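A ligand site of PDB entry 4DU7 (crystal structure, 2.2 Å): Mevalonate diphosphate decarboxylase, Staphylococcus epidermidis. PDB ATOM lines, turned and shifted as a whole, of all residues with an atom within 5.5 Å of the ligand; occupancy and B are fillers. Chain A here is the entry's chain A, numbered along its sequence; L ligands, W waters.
Merely in contact with the ligand: Ala 19 (3.2 Å), Lys 22 (3.8 Å), Trp 24 (3.7 Å), Ile 32 (3.6 Å), Met 201 (3.5 Å) and Ala 289 (3.99 Å).
Hydrophobic or aromatic side chains that line the ligand: Ala 19, Tyr 23, Trp 24, Ile 32 and Met 201.
Within 4 Å of the ligand: Ala 19, Lys 22, Tyr 23, Trp 24, Lys 26, Ile 32, Ser 112, Ser 144, Gly 145, Ser 146, Arg 149, Ser 197, Arg 198, Met 201, Asp 288 and Ala 289.
The nearest printed residue that does not touch the ligand is Met 248 (4.3 Å).
OG of Ser 144 is in hydrogen-bond range of OG of Ser 112 (3.3 Å).
The side-chain sulfur (SD) of Met 201 sits at hydrogen-bond distance from the side-chain hydroxyl (OH) of Tyr 23.
The side-chain hydroxyl (OH) of Tyr 23 sits at hydrogen-bond distance from the side-chain amino group (NZ) of Lys 26, at 2.6 Å.
The guanidinium group of Arg 149 lies within hydrogen-bond range of the side-chain amide oxygen of Asn 17 (2.7 Å).
The side-chain amino group (NZ) of Lys 22 lies within salt-bridge range of the side-chain carboxylate (OD1) of Asp 288, 2.8 Å away.
The guanidinium group of Arg 149 is in hydrogen-bond range of the side-chain hydroxyl of Ser 38, 2.9 Å away.
The guanidinium group (NH2) of Arg 198 sits at hydrogen-bond distance from the backbone carbonyl oxygen (O) of Gly 143 (3.1 Å).
The side-chain amino group (NZ) of Lys 22 lies within hydrogen-bond range of the backbone carbonyl oxygen (O) of Ala 19, 2.8 Å away.
An oxygen (O9) of the ligand lies within hydrogen-bond range of the backbone NH of Tyr 23.
OD1 of Asp 288 sits at hydrogen-bond distance from O3 of the ligand.
An oxygen (O1) of the ligand is in hydrogen-bond range of the backbone NH of Ser 146, 3.0 Å away.
The side-chain amino group of Lys 26 lies within salt-bridge range of an oxygen (O5) of the ligand (2.8 Å).
An oxygen (O2) of the ligand sits at hydrogen-bond distance from the side-chain hydroxyl (OG) of Ser 112 (3.4 Å).
O4 of the ligand lies within hydrogen-bond range of OH of Tyr 23 (2.8 Å).
The side-chain hydroxyl (OG) of Ser 146 lies within hydrogen-bond range of an oxygen (O1) of the ligand.
N of Gly 145 sits at hydrogen-bond distance from O4 of the ligand, at 2.8 Å.
The side-chain hydroxyl (OG) of Ser 144 lies within hydrogen-bond range of an oxygen (O6) of the ligand (2.5 Å).
The guanidinium group of Arg 149 is in salt-bridge range of an oxygen (O10) of the ligand (2.9 Å).
The side-chain hydroxyl (OG) of Ser 197 is in hydrogen-bond range of an oxygen (O2) of the ligand, at 2.9 Å.
O5 of the ligand is in salt-bridge range of NE of Arg 198, 2.8 Å away.
Water W1 bridges an oxygen (O6) of the ligand (2.5 Å) and the side-chain hydroxyl of Ser 144 (3.4 Å).
Water W2 lies within hydrogen-bond range of the backbone NH of Ala 19 (2.8 Å), the side-chain carboxylate of Asp 288 (3.0 Å) and an oxygen (O10) of the ligand (3.0 Å).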
ATOM      1  N   ASN A  17     -24.977 -36.191  -4.918  1.00  0.00           N
ATOM      2  CA  ASN A  17     -25.889 -36.615  -5.976  1.00  0.00           C
ATOM      3  C   ASN A  17     -25.499 -35.968  -7.291  1.00  0.00           C
ATOM      4  O   ASN A  17     -25.023 -34.836  -7.303  1.00  0.00           O
ATOM      5  CB  ASN A  17     -27.352 -36.275  -5.618  1.00  0.00           C
ATOM      6  CG  ASN A  17     -27.672 -34.778  -5.752  1.00  0.00           C
ATOM      7  OD1 ASN A  17     -28.027 -34.309  -6.843  1.00  0.00           O
ATOM      8  ND2 ASN A  17     -27.569 -34.038  -4.639  1.00  0.00           N
ATOM      9  N   ALA A  19     -26.932 -34.681 -11.004  1.00  0.00           N
ATOM     10  CA  ALA A  19     -28.122 -34.359 -11.759  1.00  0.00           C
ATOM     11  C   ALA A  19     -28.130 -35.070 -13.111  1.00  0.00           C
ATOM     12  O   ALA A  19     -27.165 -34.954 -13.885  1.00  0.00           O
ATOM     13  CB  ALA A  19     -28.261 -32.862 -11.938  1.00  0.00           C
ATOM     14  N   ILE A  21     -31.136 -34.704 -14.951  1.00  0.00           N
ATOM     15  CA  ILE A  21     -31.740 -33.535 -15.564  1.00  0.00           C
ATOM     16  C   ILE A  21     -31.255 -32.309 -14.777  1.00  0.00           C
ATOM     17  O   ILE A  21     -31.501 -32.205 -13.583  1.00  0.00           O
ATOM     18  CB  ILE A  21     -33.264 -33.606 -15.570  1.00  0.00           C
ATOM     19  CG1 ILE A  21     -33.708 -34.851 -16.358  1.00  0.00           C
ATOM     20  CG2 ILE A  21     -33.848 -32.361 -16.177  1.00  0.00           C
ATOM     21  CD1 ILE A  21     -33.562 -34.687 -17.882  1.00  0.00           C
ATOM     22  N   LYS A  22     -30.585 -31.394 -15.484  1.00  0.00           N
ATOM     23  CA  LYS A  22     -29.822 -30.310 -14.848  1.00  0.00           C
ATOM     24  C   LYS A  22     -30.636 -29.179 -14.193  1.00  0.00           C
ATOM     25  O   LYS A  22     -31.603 -28.674 -14.763  1.00  0.00           O
ATOM     26  CB  LYS A  22     -28.827 -29.676 -15.853  1.00  0.00           C
ATOM     27  CG  LYS A  22     -27.839 -30.653 -16.503  1.00  0.00           C
ATOM     28  CD  LYS A  22     -27.221 -31.626 -15.501  1.00  0.00           C
ATOM     29  CE  LYS A  22     -25.879 -32.154 -15.995  1.00  0.00           C
ATOM     30  NZ  LYS A  22     -25.351 -33.327 -15.241  1.00  0.00           N
ATOM     31  N   TYR A  23     -30.208 -28.801 -12.989  1.00  0.00           N
ATOM     32  CA  TYR A  23     -30.485 -27.490 -12.428  1.00  0.00           C
ATOM     33  C   TYR A  23     -29.459 -26.516 -13.019  1.00  0.00           C
ATOM     34  O   TYR A  23     -28.259 -26.760 -12.931  1.00  0.00           O
ATOM     35  CB  TYR A  23     -30.347 -27.560 -10.897  1.00  0.00           C
ATOM     36  CG  TYR A  23     -29.971 -26.266 -10.176  1.00  0.00           C
ATOM     37  CD1 TYR A  23     -30.634 -25.078 -10.410  1.00  0.00           C
ATOM     38  CD2 TYR A  23     -28.957 -26.267  -9.211  1.00  0.00           C
ATOM     39  CE1 TYR A  23     -30.306 -23.909  -9.713  1.00  0.00           C
ATOM     40  CE2 TYR A  23     -28.631 -25.111  -8.510  1.00  0.00           C
ATOM     41  CZ  TYR A  23     -29.300 -23.946  -8.766  1.00  0.00           C
ATOM     42  OH  TYR A  23     -28.950 -22.791  -8.083  1.00  0.00           O
ATOM     43  N   TRP A  24     -29.915 -25.421 -13.616  1.00  0.00           N
ATOM     44  CA  TRP A  24     -28.971 -24.514 -14.265  1.00  0.00           C
ATOM     45  C   TRP A  24     -29.608 -23.161 -14.516  1.00  0.00           C
ATOM     46  O   TRP A  24     -30.294 -22.948 -15.533  1.00  0.00           O
ATOM     47  CB  TRP A  24     -28.465 -25.113 -15.590  1.00  0.00           C
ATOM     48  CG  TRP A  24     -27.239 -24.417 -16.073  1.00  0.00           C
ATOM     49  CD1 TRP A  24     -27.106 -23.636 -17.193  1.00  0.00           C
ATOM     50  CD2 TRP A  24     -25.965 -24.399 -15.420  1.00  0.00           C
ATOM     51  NE1 TRP A  24     -25.813 -23.152 -17.281  1.00  0.00           N
ATOM     52  CE2 TRP A  24     -25.100 -23.601 -16.203  1.00  0.00           C
ATOM     53  CE3 TRP A  24     -25.474 -24.985 -14.247  1.00  0.00           C
ATOM     54  CZ2 TRP A  24     -23.769 -23.375 -15.846  1.00  0.00           C
ATOM     55  CZ3 TRP A  24     -24.153 -24.759 -13.892  1.00  0.00           C
ATOM     56  CH2 TRP A  24     -23.316 -23.956 -14.689  1.00  0.00           C
ATOM     57  N   LYS A  26     -30.950 -19.655 -11.774  1.00  0.00           N
ATOM     58  CA  LYS A  26     -31.893 -19.357 -10.698  1.00  0.00           C
ATOM     59  C   LYS A  26     -32.973 -18.358 -11.111  1.00  0.00           C
ATOM     60  O   LYS A  26     -32.689 -17.345 -11.755  1.00  0.00           O
ATOM     61  CB  LYS A  26     -31.147 -18.780  -9.497  1.00  0.00           C
ATOM     62  CG  LYS A  26     -30.250 -19.759  -8.749  1.00  0.00           C
ATOM     63  CD  LYS A  26     -29.282 -18.977  -7.858  1.00  0.00           C
ATOM     64  CE  LYS A  26     -28.330 -19.890  -7.125  1.00  0.00           C
ATOM     65  NZ  LYS A  26     -27.437 -20.627  -8.072  1.00  0.00           N
ATOM     66  N   ILE A  32     -32.319 -19.036  -3.560  1.00  0.00           N
ATOM     67  CA  ILE A  32     -31.980 -20.203  -4.399  1.00  0.00           C
ATOM     68  C   ILE A  32     -33.215 -20.961  -4.880  1.00  0.00           C
ATOM     69  O   ILE A  32     -33.410 -22.145  -4.570  1.00  0.00           O
ATOM     70  CB  ILE A  32     -30.951 -21.127  -3.702  1.00  0.00           C
ATOM     71  CG1 ILE A  32     -29.756 -20.297  -3.217  1.00  0.00           C
ATOM     72  CG2 ILE A  32     -30.492 -22.263  -4.639  1.00  0.00           C
ATOM     73  CD1 ILE A  32     -28.551 -21.119  -2.809  1.00  0.00           C
ATOM     74  N   SER A  38     -35.231 -30.370 -11.479  1.00  0.00           N
ATOM     75  CA  SER A  38     -34.091 -31.209 -11.832  1.00  0.00           C
ATOM     76  C   SER A  38     -34.294 -32.619 -11.272  1.00  0.00           C
ATOM     77  O   SER A  38     -35.036 -32.808 -10.333  1.00  0.00           O
ATOM     78  CB  SER A  38     -32.778 -30.616 -11.292  1.00  0.00           C
ATOM     79  OG  SER A  38     -32.836 -30.386  -9.890  1.00  0.00           O
ATOM     80  N   SER A 112     -20.713 -29.450  -2.570  1.00  0.00           N
ATOM     81  CA  SER A 112     -21.780 -28.582  -2.054  1.00  0.00           C
ATOM     82  C   SER A 112     -23.066 -29.346  -1.694  1.00  0.00           C
ATOM     83  O   SER A 112     -23.659 -29.110  -0.648  1.00  0.00           O
ATOM     84  CB  SER A 112     -22.074 -27.381  -2.976  1.00  0.00           C
ATOM     85  OG  SER A 112     -22.473 -27.797  -4.283  1.00  0.00           O
ATOM     86  N   GLY A 143     -28.470 -23.269   1.227  1.00  0.00           N
ATOM     87  CA  GLY A 143     -27.022 -23.247   1.207  1.00  0.00           C
ATOM     88  C   GLY A 143     -26.507 -23.521  -0.198  1.00  0.00           C
ATOM     89  O   GLY A 143     -25.613 -22.838  -0.704  1.00  0.00           O
ATOM     90  N   SER A 144     -27.091 -24.536  -0.813  1.00  0.00           N
ATOM     91  CA  SER A 144     -26.735 -24.879  -2.190  1.00  0.00           C
ATOM     92  C   SER A 144     -27.879 -25.633  -2.831  1.00  0.00           C
ATOM     93  O   SER A 144     -28.359 -26.618  -2.278  1.00  0.00           O
ATOM     94  CB  SER A 144     -25.450 -25.713  -2.221  1.00  0.00           C
ATOM     95  OG  SER A 144     -25.007 -25.859  -3.556  1.00  0.00           O
ATOM     96  N   GLY A 145     -28.300 -25.174  -4.006  1.00  0.00           N
ATOM     97  CA  GLY A 145     -29.440 -25.742  -4.716  1.00  0.00           C
ATOM     98  C   GLY A 145     -29.415 -27.257  -4.803  1.00  0.00           C
ATOM     99  O   GLY A 145     -30.401 -27.915  -4.459  1.00  0.00           O
ATOM    100  N   SER A 146     -28.302 -27.816  -5.264  1.00  0.00           N
ATOM    101  CA  SER A 146     -28.217 -29.261  -5.397  1.00  0.00           C
ATOM    102  C   SER A 146     -28.197 -30.014  -4.055  1.00  0.00           C
ATOM    103  O   SER A 146     -28.384 -31.226  -4.016  1.00  0.00           O
ATOM    104  CB  SER A 146     -27.003 -29.670  -6.239  1.00  0.00           C
ATOM    105  OG  SER A 146     -25.798 -29.196  -5.675  1.00  0.00           O
ATOM    106  N   ALA A 147     -27.977 -29.276  -2.966  1.00  0.00           N
ATOM    107  CA  ALA A 147     -27.993 -29.881  -1.639  1.00  0.00           C
ATOM    108  C   ALA A 147     -29.408 -30.338  -1.269  1.00  0.00           C
ATOM    109  O   ALA A 147     -29.594 -31.279  -0.483  1.00  0.00           O
ATOM    110  CB  ALA A 147     -27.456 -28.900  -0.600  1.00  0.00           C
ATOM    111  N   ARG A 149     -31.356 -32.030  -2.823  1.00  0.00           N
ATOM    112  CA  ARG A 149     -31.654 -33.387  -3.300  1.00  0.00           C
ATOM    113  C   ARG A 149     -30.927 -34.469  -2.521  1.00  0.00           C
ATOM    114  O   ARG A 149     -31.340 -35.625  -2.520  1.00  0.00           O
ATOM    115  CB  ARG A 149     -31.364 -33.534  -4.798  1.00  0.00           C
ATOM    116  CG  ARG A 149     -31.994 -32.446  -5.669  1.00  0.00           C
ATOM    117  CD  ARG A 149     -31.728 -32.678  -7.155  1.00  0.00           C
ATOM    118  NE  ARG A 149     -30.302 -32.792  -7.458  1.00  0.00           N
ATOM    119  CZ  ARG A 149     -29.615 -31.904  -8.153  1.00  0.00           C
ATOM    120  NH1 ARG A 149     -30.243 -30.838  -8.640  1.00  0.00           N
ATOM    121  NH2 ARG A 149     -28.318 -32.089  -8.368  1.00  0.00           N
ATOM    122  N   SER A 197     -20.069 -22.991 -10.440  1.00  0.00           N
ATOM    123  CA  SER A 197     -21.434 -23.320 -10.842  1.00  0.00           C
ATOM    124  C   SER A 197     -22.394 -22.144 -10.665  1.00  0.00           C
ATOM    125  O   SER A 197     -23.137 -21.780 -11.586  1.00  0.00           O
ATOM    126  CB  SER A 197     -21.932 -24.551 -10.095  1.00  0.00           C
ATOM    127  OG  SER A 197     -21.889 -24.336  -8.692  1.00  0.00           O
ATOM    128  N   ARG A 198     -22.355 -21.527  -9.487  1.00  0.00           N
ATOM    129  CA  ARG A 198     -23.251 -20.411  -9.170  1.00  0.00           C
ATOM    130  C   ARG A 198     -23.043 -19.233 -10.109  1.00  0.00           C
ATOM    131  O   ARG A 198     -24.007 -18.609 -10.578  1.00  0.00           O
ATOM    132  CB  ARG A 198     -23.029 -19.939  -7.724  1.00  0.00           C
ATOM    133  CG  ARG A 198     -23.971 -18.806  -7.261  1.00  0.00           C
ATOM    134  CD  ARG A 198     -23.985 -18.662  -5.712  1.00  0.00           C
ATOM    135  NE  ARG A 198     -24.447 -19.882  -5.054  1.00  0.00           N
ATOM    136  CZ  ARG A 198     -24.497 -20.079  -3.730  1.00  0.00           C
ATOM    137  NH1 ARG A 198     -24.115 -19.123  -2.900  1.00  0.00           N
ATOM    138  NH2 ARG A 198     -24.937 -21.241  -3.243  1.00  0.00           N
ATOM    139  N   MET A 201     -23.765 -20.371 -14.010  1.00  0.00           N
ATOM    140  CA  MET A 201     -25.186 -20.517 -14.314  1.00  0.00           C
ATOM    141  C   MET A 201     -25.859 -19.145 -14.304  1.00  0.00           C
ATOM    142  O   MET A 201     -26.859 -18.928 -14.995  1.00  0.00           O
ATOM    143  CB  MET A 201     -25.877 -21.526 -13.385  1.00  0.00           C
ATOM    144  CG  MET A 201     -26.225 -21.017 -11.984  1.00  0.00           C
ATOM    145  SD  MET A 201     -27.337 -22.107 -11.037  1.00  0.00           S
ATOM    146  CE  MET A 201     -26.331 -23.565 -10.812  1.00  0.00           C
ATOM    147  N   MET A 248     -27.636 -28.325 -21.647  1.00  0.00           N
ATOM    148  CA  MET A 248     -27.165 -27.436 -20.585  1.00  0.00           C
ATOM    149  C   MET A 248     -25.824 -26.794 -20.982  1.00  0.00           C
ATOM    150  O   MET A 248     -25.605 -25.582 -20.802  1.00  0.00           O
ATOM    151  CB  MET A 248     -26.974 -28.233 -19.288  1.00  0.00           C
ATOM    152  CG  MET A 248     -26.800 -27.357 -18.052  1.00  0.00           C
ATOM    153  SD  MET A 248     -25.393 -27.856 -17.048  1.00  0.00           S
ATOM    154  CE  MET A 248     -24.060 -27.061 -17.946  1.00  0.00           C
ATOM    155  N   MET A 287     -22.248 -34.289 -17.800  1.00  0.00           N
ATOM    156  CA  MET A 287     -21.176 -33.460 -17.259  1.00  0.00           C
ATOM    157  C   MET A 287     -21.787 -32.312 -16.491  1.00  0.00           C
ATOM    158  O   MET A 287     -22.885 -31.830 -16.839  1.00  0.00           O
ATOM    159  CB  MET A 287     -20.284 -32.902 -18.377  1.00  0.00           C
ATOM    160  CG  MET A 287     -19.407 -33.949 -19.036  1.00  0.00           C
ATOM    161  SD  MET A 287     -20.284 -34.815 -20.376  1.00  0.00           S
ATOM    162  CE  MET A 287     -21.076 -33.451 -21.224  1.00  0.00           C
ATOM    163  N   ASP A 288     -21.082 -31.854 -15.466  1.00  0.00           N
ATOM    164  CA  ASP A 288     -21.561 -30.709 -14.697  1.00  0.00           C
ATOM    165  C   ASP A 288     -20.683 -29.472 -14.898  1.00  0.00           C
ATOM    166  O   ASP A 288     -20.340 -29.152 -16.040  1.00  0.00           O
ATOM    167  CB  ASP A 288     -21.701 -31.102 -13.225  1.00  0.00           C
ATOM    168  CG  ASP A 288     -22.745 -32.174 -13.045  1.00  0.00           C
ATOM    169  OD1 ASP A 288     -23.926 -31.877 -13.293  1.00  0.00           O
ATOM    170  OD2 ASP A 288     -22.398 -33.327 -12.697  1.00  0.00           O
ATOM    171  N   ALA A 289     -20.330 -28.787 -13.820  1.00  0.00           N
ATOM    172  CA  ALA A 289     -19.592 -27.528 -13.925  1.00  0.00           C
ATOM    173  C   ALA A 289     -18.100 -27.781 -13.989  1.00  0.00           C
ATOM    174  O   ALA A 289     -17.321 -27.253 -13.198  1.00  0.00           O
ATOM    175  CB  ALA A 289     -19.916 -26.609 -12.739  1.00  0.00           C
HETATM  176  C1  LIG L   1     -24.215 -28.370 -12.993  1.00  0.00           C
HETATM  177  O1  LIG L   1     -25.909 -26.690  -6.716  1.00  0.00           O
HETATM  178  O2  LIG L   1     -23.580 -25.858  -6.826  1.00  0.00           O
HETATM  179  O3  LIG L   1     -24.232 -29.486 -10.966  1.00  0.00           O
HETATM  180  O4  LIG L   1     -27.276 -23.407  -5.927  1.00  0.00           O
HETATM  181  O5  LIG L   1     -25.461 -21.940  -6.629  1.00  0.00           O
HETATM  182  O6  LIG L   1     -25.018 -23.772  -5.013  1.00  0.00           O
HETATM  183  P1  LIG L   1     -25.797 -23.352  -6.229  1.00  0.00           P
HETATM  184  O7  LIG L   1     -25.466 -24.273  -7.459  1.00  0.00           O
HETATM  185  P2  LIG L   1     -24.952 -25.749  -7.436  1.00  0.00           P
HETATM  186  O8  LIG L   1     -24.884 -26.090  -8.956  1.00  0.00           O
HETATM  187  C2  LIG L   1     -25.145 -27.315  -9.521  1.00  0.00           C
HETATM  188  C3  LIG L   1     -25.179 -27.331 -11.018  1.00  0.00           C
HETATM  189  C4  LIG L   1     -24.976 -28.622 -11.729  1.00  0.00           C
HETATM  190  C5  LIG L   1     -26.308 -29.227 -12.054  1.00  0.00           C
HETATM  191  C6  LIG L   1     -27.173 -29.808 -10.976  1.00  0.00           C
HETATM  192  O9  LIG L   1     -28.426 -29.784 -11.122  1.00  0.00           O
HETATM  193  O10 LIG L   1     -26.666 -30.339  -9.943  1.00  0.00           O
HETATM  194  O   HOH W   1     -22.566 -24.022  -4.986  1.00  0.00           O
HETATM  195  O   HOH W   2     -24.902 -32.723 -10.611  1.00  0.00           O
